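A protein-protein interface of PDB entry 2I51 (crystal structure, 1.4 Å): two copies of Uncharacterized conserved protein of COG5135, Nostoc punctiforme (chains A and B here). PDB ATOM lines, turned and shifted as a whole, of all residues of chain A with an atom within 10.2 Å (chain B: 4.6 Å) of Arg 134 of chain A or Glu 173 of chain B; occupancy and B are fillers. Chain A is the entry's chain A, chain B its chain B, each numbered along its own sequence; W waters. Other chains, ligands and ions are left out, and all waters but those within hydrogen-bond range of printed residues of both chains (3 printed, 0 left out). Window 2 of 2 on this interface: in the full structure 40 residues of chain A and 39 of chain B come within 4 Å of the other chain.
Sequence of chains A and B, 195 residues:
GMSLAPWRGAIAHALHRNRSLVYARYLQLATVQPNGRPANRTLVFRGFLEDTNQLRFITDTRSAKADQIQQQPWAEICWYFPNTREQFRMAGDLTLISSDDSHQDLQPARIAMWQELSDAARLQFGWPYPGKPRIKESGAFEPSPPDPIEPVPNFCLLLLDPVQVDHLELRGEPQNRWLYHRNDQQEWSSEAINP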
ATOM      1  N   TRP A 127      -7.987 -22.274 -19.745  1.00  0.00           N
ATOM      2  CA  TRP A 127      -8.368 -21.002 -19.112  1.00  0.00           C
ATOM      3  C   TRP A 127      -9.085 -21.219 -17.775  1.00  0.00           C
ATOM      4  O   TRP A 127      -9.545 -22.312 -17.467  1.00  0.00           O
ATOM      5  CB  TRP A 127      -9.272 -20.203 -20.052  1.00  0.00           C
ATOM      6  CG  TRP A 127      -8.579 -19.580 -21.223  1.00  0.00           C
ATOM      7  CD1 TRP A 127      -7.259 -19.662 -21.554  1.00  0.00           C
ATOM      8  CD2 TRP A 127      -9.193 -18.773 -22.219  1.00  0.00           C
ATOM      9  NE1 TRP A 127      -7.025 -18.965 -22.714  1.00  0.00           N
ATOM     10  CE2 TRP A 127      -8.203 -18.405 -23.141  1.00  0.00           C
ATOM     11  CE3 TRP A 127     -10.508 -18.337 -22.423  1.00  0.00           C
ATOM     12  CZ2 TRP A 127      -8.460 -17.606 -24.229  1.00  0.00           C
ATOM     13  CZ3 TRP A 127     -10.772 -17.574 -23.527  1.00  0.00           C
ATOM     14  CH2 TRP A 127      -9.749 -17.188 -24.403  1.00  0.00           C
ATOM     15  N   PRO A 128      -9.105 -20.187 -16.919  1.00  0.00           N
ATOM     16  CA  PRO A 128      -9.780 -20.364 -15.647  1.00  0.00           C
ATOM     17  C   PRO A 128     -11.265 -20.617 -15.761  1.00  0.00           C
ATOM     18  O   PRO A 128     -11.838 -20.412 -16.820  1.00  0.00           O
ATOM     19  CB  PRO A 128      -9.491 -19.056 -14.892  1.00  0.00           C
ATOM     20  CG  PRO A 128      -8.971 -18.122 -15.865  1.00  0.00           C
ATOM     21  CD  PRO A 128      -8.451 -18.884 -17.057  1.00  0.00           C
ATOM     22  N   TYR A 129     -11.841 -21.095 -14.662  1.00  0.00           N
ATOM     23  CA  TYR A 129     -13.194 -21.630 -14.605  1.00  0.00           C
ATOM     24  C   TYR A 129     -14.233 -20.634 -15.151  1.00  0.00           C
ATOM     25  O   TYR A 129     -14.405 -19.558 -14.613  1.00  0.00           O
ATOM     26  CB  TYR A 129     -13.554 -22.000 -13.174  1.00  0.00           C
ATOM     27  CG  TYR A 129     -14.587 -23.084 -13.068  1.00  0.00           C
ATOM     28  CD1 TYR A 129     -15.909 -22.843 -13.392  1.00  0.00           C
ATOM     29  CD2 TYR A 129     -14.248 -24.348 -12.636  1.00  0.00           C
ATOM     30  CE1 TYR A 129     -16.869 -23.841 -13.293  1.00  0.00           C
ATOM     31  CE2 TYR A 129     -15.209 -25.356 -12.537  1.00  0.00           C
ATOM     32  CZ  TYR A 129     -16.504 -25.085 -12.876  1.00  0.00           C
ATOM     33  OH  TYR A 129     -17.476 -26.057 -12.793  1.00  0.00           O
ATOM     34  N   PRO A 130     -14.908 -20.998 -16.243  1.00  0.00           N
ATOM     35  CA  PRO A 130     -15.829 -20.066 -16.865  1.00  0.00           C
ATOM     36  C   PRO A 130     -16.929 -19.623 -15.925  1.00  0.00           C
ATOM     37  O   PRO A 130     -17.472 -20.436 -15.159  1.00  0.00           O
ATOM     38  CB  PRO A 130     -16.422 -20.869 -18.024  1.00  0.00           C
ATOM     39  CG  PRO A 130     -16.233 -22.257 -17.671  1.00  0.00           C
ATOM     40  CD  PRO A 130     -14.903 -22.292 -16.936  1.00  0.00           C
ATOM     41  N   GLY A 131     -17.246 -18.331 -15.976  1.00  0.00           N
ATOM     42  CA  GLY A 131     -18.311 -17.755 -15.151  1.00  0.00           C
ATOM     43  C   GLY A 131     -17.956 -17.301 -13.744  1.00  0.00           C
ATOM     44  O   GLY A 131     -18.756 -16.669 -13.077  1.00  0.00           O
ATOM     45  N   LYS A 132     -16.768 -17.622 -13.266  1.00  0.00           N
ATOM     46  CA  LYS A 132     -16.370 -17.185 -11.956  1.00  0.00           C
ATOM     47  C   LYS A 132     -15.827 -15.774 -12.072  1.00  0.00           C
ATOM     48  O   LYS A 132     -15.564 -15.327 -13.155  1.00  0.00           O
ATOM     49  CB  LYS A 132     -15.302 -18.137 -11.394  1.00  0.00           C
ATOM     50  CG  LYS A 132     -15.781 -19.575 -11.251  1.00  0.00           C
ATOM     51  CD  LYS A 132     -17.016 -19.705 -10.405  1.00  0.00           C
ATOM     52  CE  LYS A 132     -17.329 -21.172 -10.109  1.00  0.00           C
ATOM     53  NZ  LYS A 132     -18.309 -21.302  -9.003  1.00  0.00           N
ATOM     54  N   PRO A 133     -15.640 -15.070 -10.940  1.00  0.00           N
ATOM     55  CA  PRO A 133     -15.048 -13.732 -10.977  1.00  0.00           C
ATOM     56  C   PRO A 133     -13.768 -13.643 -11.782  1.00  0.00           C
ATOM     57  O   PRO A 133     -12.890 -14.491 -11.635  1.00  0.00           O
ATOM     58  CB  PRO A 133     -14.768 -13.460  -9.493  1.00  0.00           C
ATOM     59  CG  PRO A 133     -15.964 -14.146  -8.817  1.00  0.00           C
ATOM     60  CD  PRO A 133     -16.012 -15.452  -9.553  1.00  0.00           C
ATOM     61  N   ARG A 134     -13.659 -12.624 -12.625  1.00  0.00           N
ATOM     62  CA  ARG A 134     -12.596 -12.535 -13.625  1.00  0.00           C
ATOM     63  C   ARG A 134     -11.229 -12.493 -12.945  1.00  0.00           C
ATOM     64  O   ARG A 134     -10.985 -11.645 -12.080  1.00  0.00           O
ATOM     65  CB  ARG A 134     -12.771 -11.289 -14.483  1.00  0.00           C
ATOM     66  CG  ARG A 134     -11.601 -11.008 -15.460  1.00  0.00           C
ATOM     67  CD  ARG A 134     -11.271 -12.193 -16.308  1.00  0.00           C
ATOM     68  NE  ARG A 134     -10.137 -11.931 -17.159  1.00  0.00           N
ATOM     69  CZ  ARG A 134     -10.168 -11.530 -18.418  1.00  0.00           C
ATOM     70  NH1 ARG A 134     -11.324 -11.279 -19.022  1.00  0.00           N
ATOM     71  NH2 ARG A 134      -9.011 -11.376 -19.068  1.00  0.00           N
ATOM     72  N   ILE A 135     -10.368 -13.442 -13.306  1.00  0.00           N
ATOM     73  CA  ILE A 135      -8.963 -13.425 -12.906  1.00  0.00           C
ATOM     74  C   ILE A 135      -8.303 -12.248 -13.624  1.00  0.00           C
ATOM     75  O   ILE A 135      -8.332 -12.181 -14.846  1.00  0.00           O
ATOM     76  CB  ILE A 135      -8.295 -14.742 -13.290  1.00  0.00           C
ATOM     77  CG1 ILE A 135      -8.861 -15.892 -12.437  1.00  0.00           C
ATOM     78  CG2 ILE A 135      -6.757 -14.668 -13.123  1.00  0.00           C
ATOM     79  CD1 ILE A 135      -8.553 -15.742 -10.948  1.00  0.00           C
ATOM     80  N   LYS A 136      -7.647 -11.367 -12.867  1.00  0.00           N
ATOM     81  CA  LYS A 136      -7.136 -10.103 -13.435  1.00  0.00           C
ATOM     82  C   LYS A 136      -5.732 -10.220 -14.047  1.00  0.00           C
ATOM     83  O   LYS A 136      -5.333  -9.354 -14.841  1.00  0.00           O
ATOM     84  CB  LYS A 136      -7.123  -9.004 -12.389  1.00  0.00           C
ATOM     85  CG  LYS A 136      -8.507  -8.483 -12.010  1.00  0.00           C
ATOM     86  CD  LYS A 136      -8.372  -7.476 -10.846  1.00  0.00           C
ATOM     87  CE  LYS A 136      -9.719  -7.027 -10.313  1.00  0.00           C
ATOM     88  NZ  LYS A 136     -10.434  -8.132  -9.597  1.00  0.00           N
ATOM     89  N   GLU A 137      -5.008 -11.286 -13.724  1.00  0.00           N
ATOM     90  CA  GLU A 137      -3.664 -11.475 -14.264  1.00  0.00           C
ATOM     91  C   GLU A 137      -3.730 -12.152 -15.641  1.00  0.00           C
ATOM     92  O   GLU A 137      -4.331 -13.221 -15.798  1.00  0.00           O
ATOM     93  CB  GLU A 137      -2.799 -12.294 -13.304  1.00  0.00           C
ATOM     94  CG  GLU A 137      -2.501 -11.551 -11.996  1.00  0.00           C
ATOM     95  CD  GLU A 137      -3.720 -11.416 -11.072  1.00  0.00           C
ATOM     96  OE1 GLU A 137      -4.619 -12.291 -11.154  1.00  0.00           O
ATOM     97  OE2 GLU A 137      -3.770 -10.442 -10.265  1.00  0.00           O
ATOM     98  N   SER A 138      -3.081 -11.535 -16.631  1.00  0.00           N
ATOM     99  CA  SER A 138      -3.104 -12.035 -18.008  1.00  0.00           C
ATOM    100  C   SER A 138      -2.497 -13.437 -18.114  1.00  0.00           C
ATOM    101  O   SER A 138      -2.853 -14.199 -19.020  1.00  0.00           O
ATOM    102  N   GLY A 139      -1.587 -13.761 -17.193  1.00  0.00           N
ATOM    103  CA  GLY A 139      -0.905 -15.053 -17.180  1.00  0.00           C
ATOM    104  C   GLY A 139      -1.828 -16.266 -17.179  1.00  0.00           C
ATOM    105  O   GLY A 139      -1.537 -17.267 -17.834  1.00  0.00           O
ATOM    106  N   ALA A 140      -2.946 -16.158 -16.451  1.00  0.00           N
ATOM    107  CA  ALA A 140      -3.927 -17.243 -16.322  1.00  0.00           C
ATOM    108  C   ALA A 140      -4.551 -17.595 -17.662  1.00  0.00           C
ATOM    109  O   ALA A 140      -5.066 -18.680 -17.833  1.00  0.00           O
ATOM    110  CB  ALA A 140      -5.023 -16.850 -15.335  1.00  0.00           C
ATOM    111  N   PHE A 141      -4.488 -16.666 -18.617  1.00  0.00           N
ATOM    112  CA  PHE A 141      -5.053 -16.864 -19.948  1.00  0.00           C
ATOM    113  C   PHE A 141      -4.018 -17.215 -21.005  1.00  0.00           C
ATOM    114  O   PHE A 141      -4.367 -17.369 -22.181  1.00  0.00           O
ATOM    115  CB  PHE A 141      -5.867 -15.623 -20.338  1.00  0.00           C
ATOM    116  CG  PHE A 141      -7.086 -15.472 -19.500  1.00  0.00           C
ATOM    117  CD1 PHE A 141      -8.258 -16.115 -19.863  1.00  0.00           C
ATOM    118  CD2 PHE A 141      -7.067 -14.741 -18.315  1.00  0.00           C
ATOM    119  CE1 PHE A 141      -9.385 -16.046 -19.083  1.00  0.00           C
ATOM    120  CE2 PHE A 141      -8.181 -14.678 -17.528  1.00  0.00           C
ATOM    121  CZ  PHE A 141      -9.366 -15.318 -17.933  1.00  0.00           C
ATOM    122  N   GLU A 142      -2.778 -17.420 -20.553  1.00  0.00           N
ATOM    123  CA  GLU A 142      -1.634 -17.754 -21.404  1.00  0.00           C
ATOM    124  C   GLU A 142      -0.961 -19.027 -20.933  1.00  0.00           C
ATOM    125  O   GLU A 142       0.236 -19.061 -20.766  1.00  0.00           O
ATOM    126  CB  GLU A 142      -0.605 -16.604 -21.354  1.00  0.00           C
ATOM    127  CG  GLU A 142      -1.179 -15.272 -21.828  1.00  0.00           C
ATOM    128  CD  GLU A 142      -0.238 -14.088 -21.660  1.00  0.00           C
ATOM    129  OE1 GLU A 142       0.768 -14.190 -20.923  1.00  0.00           O
ATOM    130  OE2 GLU A 142      -0.551 -13.023 -22.242  1.00  0.00           O
ATOM    131  N   GLY B 172     -10.637  -8.971 -26.623  1.00  0.00           N
ATOM    132  CA  GLY B 172     -10.183  -8.489 -25.324  1.00  0.00           C
ATOM    133  C   GLY B 172      -8.754  -8.882 -25.043  1.00  0.00           C
ATOM    134  O   GLY B 172      -7.926  -8.974 -25.958  1.00  0.00           O
ATOM    135  N   GLU B 173      -8.473  -9.128 -23.771  1.00  0.00           N
ATOM    136  CA  GLU B 173      -7.136  -9.523 -23.305  1.00  0.00           C
ATOM    137  C   GLU B 173      -7.259 -10.761 -22.420  1.00  0.00           C
ATOM    138  O   GLU B 173      -7.000 -10.725 -21.212  1.00  0.00           O
ATOM    139  CB  GLU B 173      -6.453  -8.383 -22.528  1.00  0.00           C
ATOM    140  CG  GLU B 173      -5.600  -7.460 -23.397  1.00  0.00           C
ATOM    141  CD  GLU B 173      -6.398  -6.422 -24.139  1.00  0.00           C
ATOM    142  OE1 GLU B 173      -7.525  -6.096 -23.700  1.00  0.00           O
ATOM    143  OE2 GLU B 173      -5.887  -5.923 -25.166  1.00  0.00           O
ATOM    144  N   PRO B 174      -7.636 -11.890 -23.019  1.00  0.00           N
ATOM    145  CA  PRO B 174      -7.920 -12.152 -24.422  1.00  0.00           C
ATOM    146  C   PRO B 174      -9.391 -11.962 -24.867  1.00  0.00           C
ATOM    147  O   PRO B 174      -9.636 -11.685 -26.055  1.00  0.00           O
ATOM    148  CB  PRO B 174      -7.503 -13.614 -24.563  1.00  0.00           C
ATOM    149  CG  PRO B 174      -7.964 -14.209 -23.250  1.00  0.00           C
ATOM    150  CD  PRO B 174      -7.652 -13.121 -22.205  1.00  0.00           C
ATOM    151  N   GLN B 175     -10.310 -12.061 -23.914  1.00  0.00           N
ATOM    152  CA  GLN B 175     -11.749 -11.838 -24.106  1.00  0.00           C
ATOM    153  C   GLN B 175     -12.252 -11.149 -22.851  1.00  0.00           C
ATOM    154  O   GLN B 175     -11.628 -11.265 -21.788  1.00  0.00           O
ATOM    155  CB  GLN B 175     -12.463 -13.177 -24.285  1.00  0.00           C
ATOM    156  CG  GLN B 175     -11.995 -13.957 -25.517  1.00  0.00           C
ATOM    157  CD  GLN B 175     -12.765 -15.252 -25.762  1.00  0.00           C
ATOM    158  OE1 GLN B 175     -12.537 -15.926 -26.797  1.00  0.00           O
ATOM    159  NE2 GLN B 175     -13.657 -15.614 -24.876  1.00  0.00           N
ATOM    160  N   ASN B 176     -13.329 -10.378 -22.956  1.00  0.00           N
ATOM    161  CA  ASN B 176     -13.960  -9.813 -21.772  1.00  0.00           C
ATOM    162  C   ASN B 176     -15.343 -10.376 -21.654  1.00  0.00           C
ATOM    163  O   ASN B 176     -16.028 -10.551 -22.661  1.00  0.00           O
ATOM    164  CB  ASN B 176     -14.070  -8.305 -21.886  1.00  0.00           C
ATOM    165  CG  ASN B 176     -12.755  -7.659 -22.007  1.00  0.00           C
ATOM    166  OD1 ASN B 176     -11.867  -7.941 -21.215  1.00  0.00           O
ATOM    167  ND2 ASN B 176     -12.612  -6.780 -22.984  1.00  0.00           N
ATOM    168  N   ALA B 192     -17.456  -8.578 -13.709  1.00  0.00           N
ATOM    169  CA  ALA B 192     -16.569  -9.171 -14.679  1.00  0.00           C
ATOM    170  C   ALA B 192     -16.370 -10.629 -14.307  1.00  0.00           C
ATOM    171  O   ALA B 192     -16.041 -10.955 -13.154  1.00  0.00           O
ATOM    172  CB  ALA B 192     -15.206  -8.449 -14.713  1.00  0.00           C
ATOM    173  N   ILE B 193     -16.508 -11.503 -15.322  1.00  0.00           N
ATOM    174  CA  ILE B 193     -16.446 -12.923 -15.090  1.00  0.00           C
ATOM    175  C   ILE B 193     -15.522 -13.596 -16.118  1.00  0.00           C
ATOM    176  O   ILE B 193     -15.177 -13.009 -17.140  1.00  0.00           O
ATOM    177  CB  ILE B 193     -17.823 -13.594 -15.105  1.00  0.00           C
ATOM    178  CG1 ILE B 193     -18.556 -13.347 -16.427  1.00  0.00           C
ATOM    179  CG2 ILE B 193     -18.692 -13.139 -13.930  1.00  0.00           C
ATOM    180  CD1 ILE B 193     -19.793 -14.276 -16.622  1.00  0.00           C
ATOM    181  N   ASN B 194     -15.035 -14.789 -15.789  1.00  0.00           N
ATOM    182  CA  ASN B 194     -14.123 -15.472 -16.719  1.00  0.00           C
ATOM    183  C   ASN B 194     -14.869 -15.916 -17.942  1.00  0.00           C
ATOM    184  O   ASN B 194     -15.962 -16.457 -17.826  1.00  0.00           O
ATOM    185  CB  ASN B 194     -13.487 -16.717 -16.130  1.00  0.00           C
ATOM    186  CG  ASN B 194     -12.556 -16.409 -15.013  1.00  0.00           C
ATOM    187  OD1 ASN B 194     -11.773 -15.428 -15.040  1.00  0.00           O
ATOM    188  ND2 ASN B 194     -12.563 -17.292 -14.035  1.00  0.00           N
ATOM    189  N   PRO B 195     -14.303 -15.658 -19.110  1.00  0.00           N
ATOM    190  CA  PRO B 195     -14.939 -16.108 -20.374  1.00  0.00           C
ATOM    191  C   PRO B 195     -15.328 -17.572 -20.386  1.00  0.00           C
ATOM    192  O   PRO B 195     -14.538 -18.408 -19.950  1.00  0.00           O
ATOM    193  CB  PRO B 195     -13.882 -15.810 -21.427  1.00  0.00           C
ATOM    194  CG  PRO B 195     -12.966 -14.823 -20.834  1.00  0.00           C
ATOM    195  CD  PRO B 195     -13.076 -14.880 -19.344  1.00  0.00           C
ATOM    196  OXT PRO B 195     -16.440 -17.965 -20.832  1.00  0.00           O
HETATM  197  O   HOH W   1      -9.465  -9.105 -21.109  1.00  0.00           O
HETATM  198  O   HOH W   2     -14.020 -10.780 -18.077  1.00  0.00           O
HETATM  199  O   HOH W   3     -12.143 -18.395 -18.728  1.00  0.00           O
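The backbone NH (N) of Arg 134 of chain A sits at hydrogen-bond distance from the backbone carbonyl oxygen (O) of Ala 192 of chain B (3.0 Å).
The backbone carbonyl oxygen (O) of Asn 194 of chain B is in hydrogen-bond range of the backbone NH (N) of Gly 131 of chain A (2.9 Å).
N of Asn 194 of chain B lies within hydrogen-bond range of O of Lys 132 of chain A (2.7 Å).
The guanidinium group (NH2) of Arg 134 of chain A is in hydrogen-bond range of the backbone carbonyl oxygen (O) of Glu 173 of chain B (3.0 Å).
The guanidinium group of Arg 134 of chain A lies within hydrogen-bond range of the backbone carbonyl oxygen of Gln 175 of chain B (2.8 Å).
O of Tyr 129 of chain A sits at hydrogen-bond distance from ND2 of Asn 194 of chain B (3.0 Å).
N of Ile 135 of chain A is in hydrogen-bond range of OD1 of Asn 194 of chain B (3.0 Å).
The backbone carbonyl oxygen of Phe 141 of chain A sits at hydrogen-bond distance from the indole nitrogen of Trp 127 of chain A (3.1 Å).
CZ2 of Trp 127 of chain A touches CG of Pro 174 of chain B, at 3.6 Å.
Gln 175 of chain B touches Trp 127 of chain A.
Lys 132 of chain A touches Ile 193 of chain B (O to CA, 3.2 Å).
Pro 133 of chain A touches Ala 192 of chain B (CA to O, 3.7 Å).
Pro 174 of chain B touches Arg 134 of chain A (CD to NH2, 3.8 Å).
N of Arg 134 of chain A touches CA of Ile 193 of chain B, at 3.7 Å.
Arg 134 of chain A touches Asn 194 of chain B (CA to OD1, 3.3 Å).
Phe 141 of chain A touches Pro 174 of chain B (CB to CD, 3.6 Å).
Phe 141 of chain A touches Asn 194 of chain B (CZ to OD1, 3.8 Å).
Phe 141 of chain A touches Pro 195 of chain B (CE1 to CD, 3.9 Å).
Printed residues of chain B within 4 Å of Tyr 129 of chain A: Asn 194.
Printed residues of chain B within 4 Å of Arg 134 of chain A: Glu 173 (3.0 Å), Pro 174 (3.8 Å), Gln 175 (2.8 Å), Ala 192 (3.0 Å), Ile 193 (3.7 Å) and Asn 194 (3.3 Å).
Of the printed residues of chain B, Ile 135 of chain A touches Asn 194 (3.0 Å).
No residue of chain A comes within 4 Å of Gly 172 of chain B.
Glu 173 of chain B touches just one residue of chain A: Arg 134 (3.0 Å).
Of chain A, only Trp 127 (3.6 Å), Arg 134 (3.8 Å) and Phe 141 (3.6 Å) come within 4 Å of Pro 174 of chain B.
Of the printed residues of chain A, Gln 175 of chain B touches Trp 127 and Arg 134.
No residue of chain A comes within 4 Å of Asn 176 of chain B.
Ala 192 of chain B touches just these residues of chain A: Pro 133 (3.7 Å) and Arg 134 (3.0 Å).
Printed residues of chain A within 4 Å of Asn 194 of chain B: Pro 128, Tyr 129, Pro 130, Gly 131, Lys 132, Pro 133, Arg 134, Ile 135 and Phe 141.
Of the 9 printed residues of chain B, 7 touch a printed residue of chain A.
Among the printed residues, 22 pairs touch across the chains.
No position is printed for both chains.
Of the 22 pairs that touch across the chains among the printed residues, none has its exchanged pair printed and touching as well.
Water W1 lies within hydrogen-bond range of OD1 of Asn 176 of chain B (2.7 Å), N of Glu 173 of chain B (2.8 Å), NH2 of Arg 134 of chain A (3.1 Å) and O of Gln 175 of chain B (3.1 Å).
Water W2 lies within hydrogen-bond range of the backbone carbonyl oxygen of Ile 193 of chain B and the guanidinium group of Arg 134 of chain A.
Water W3 bridges O of Pro 195 of chain B (2.7 Å) and O of Pro 128 of chain A (2.8 Å).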
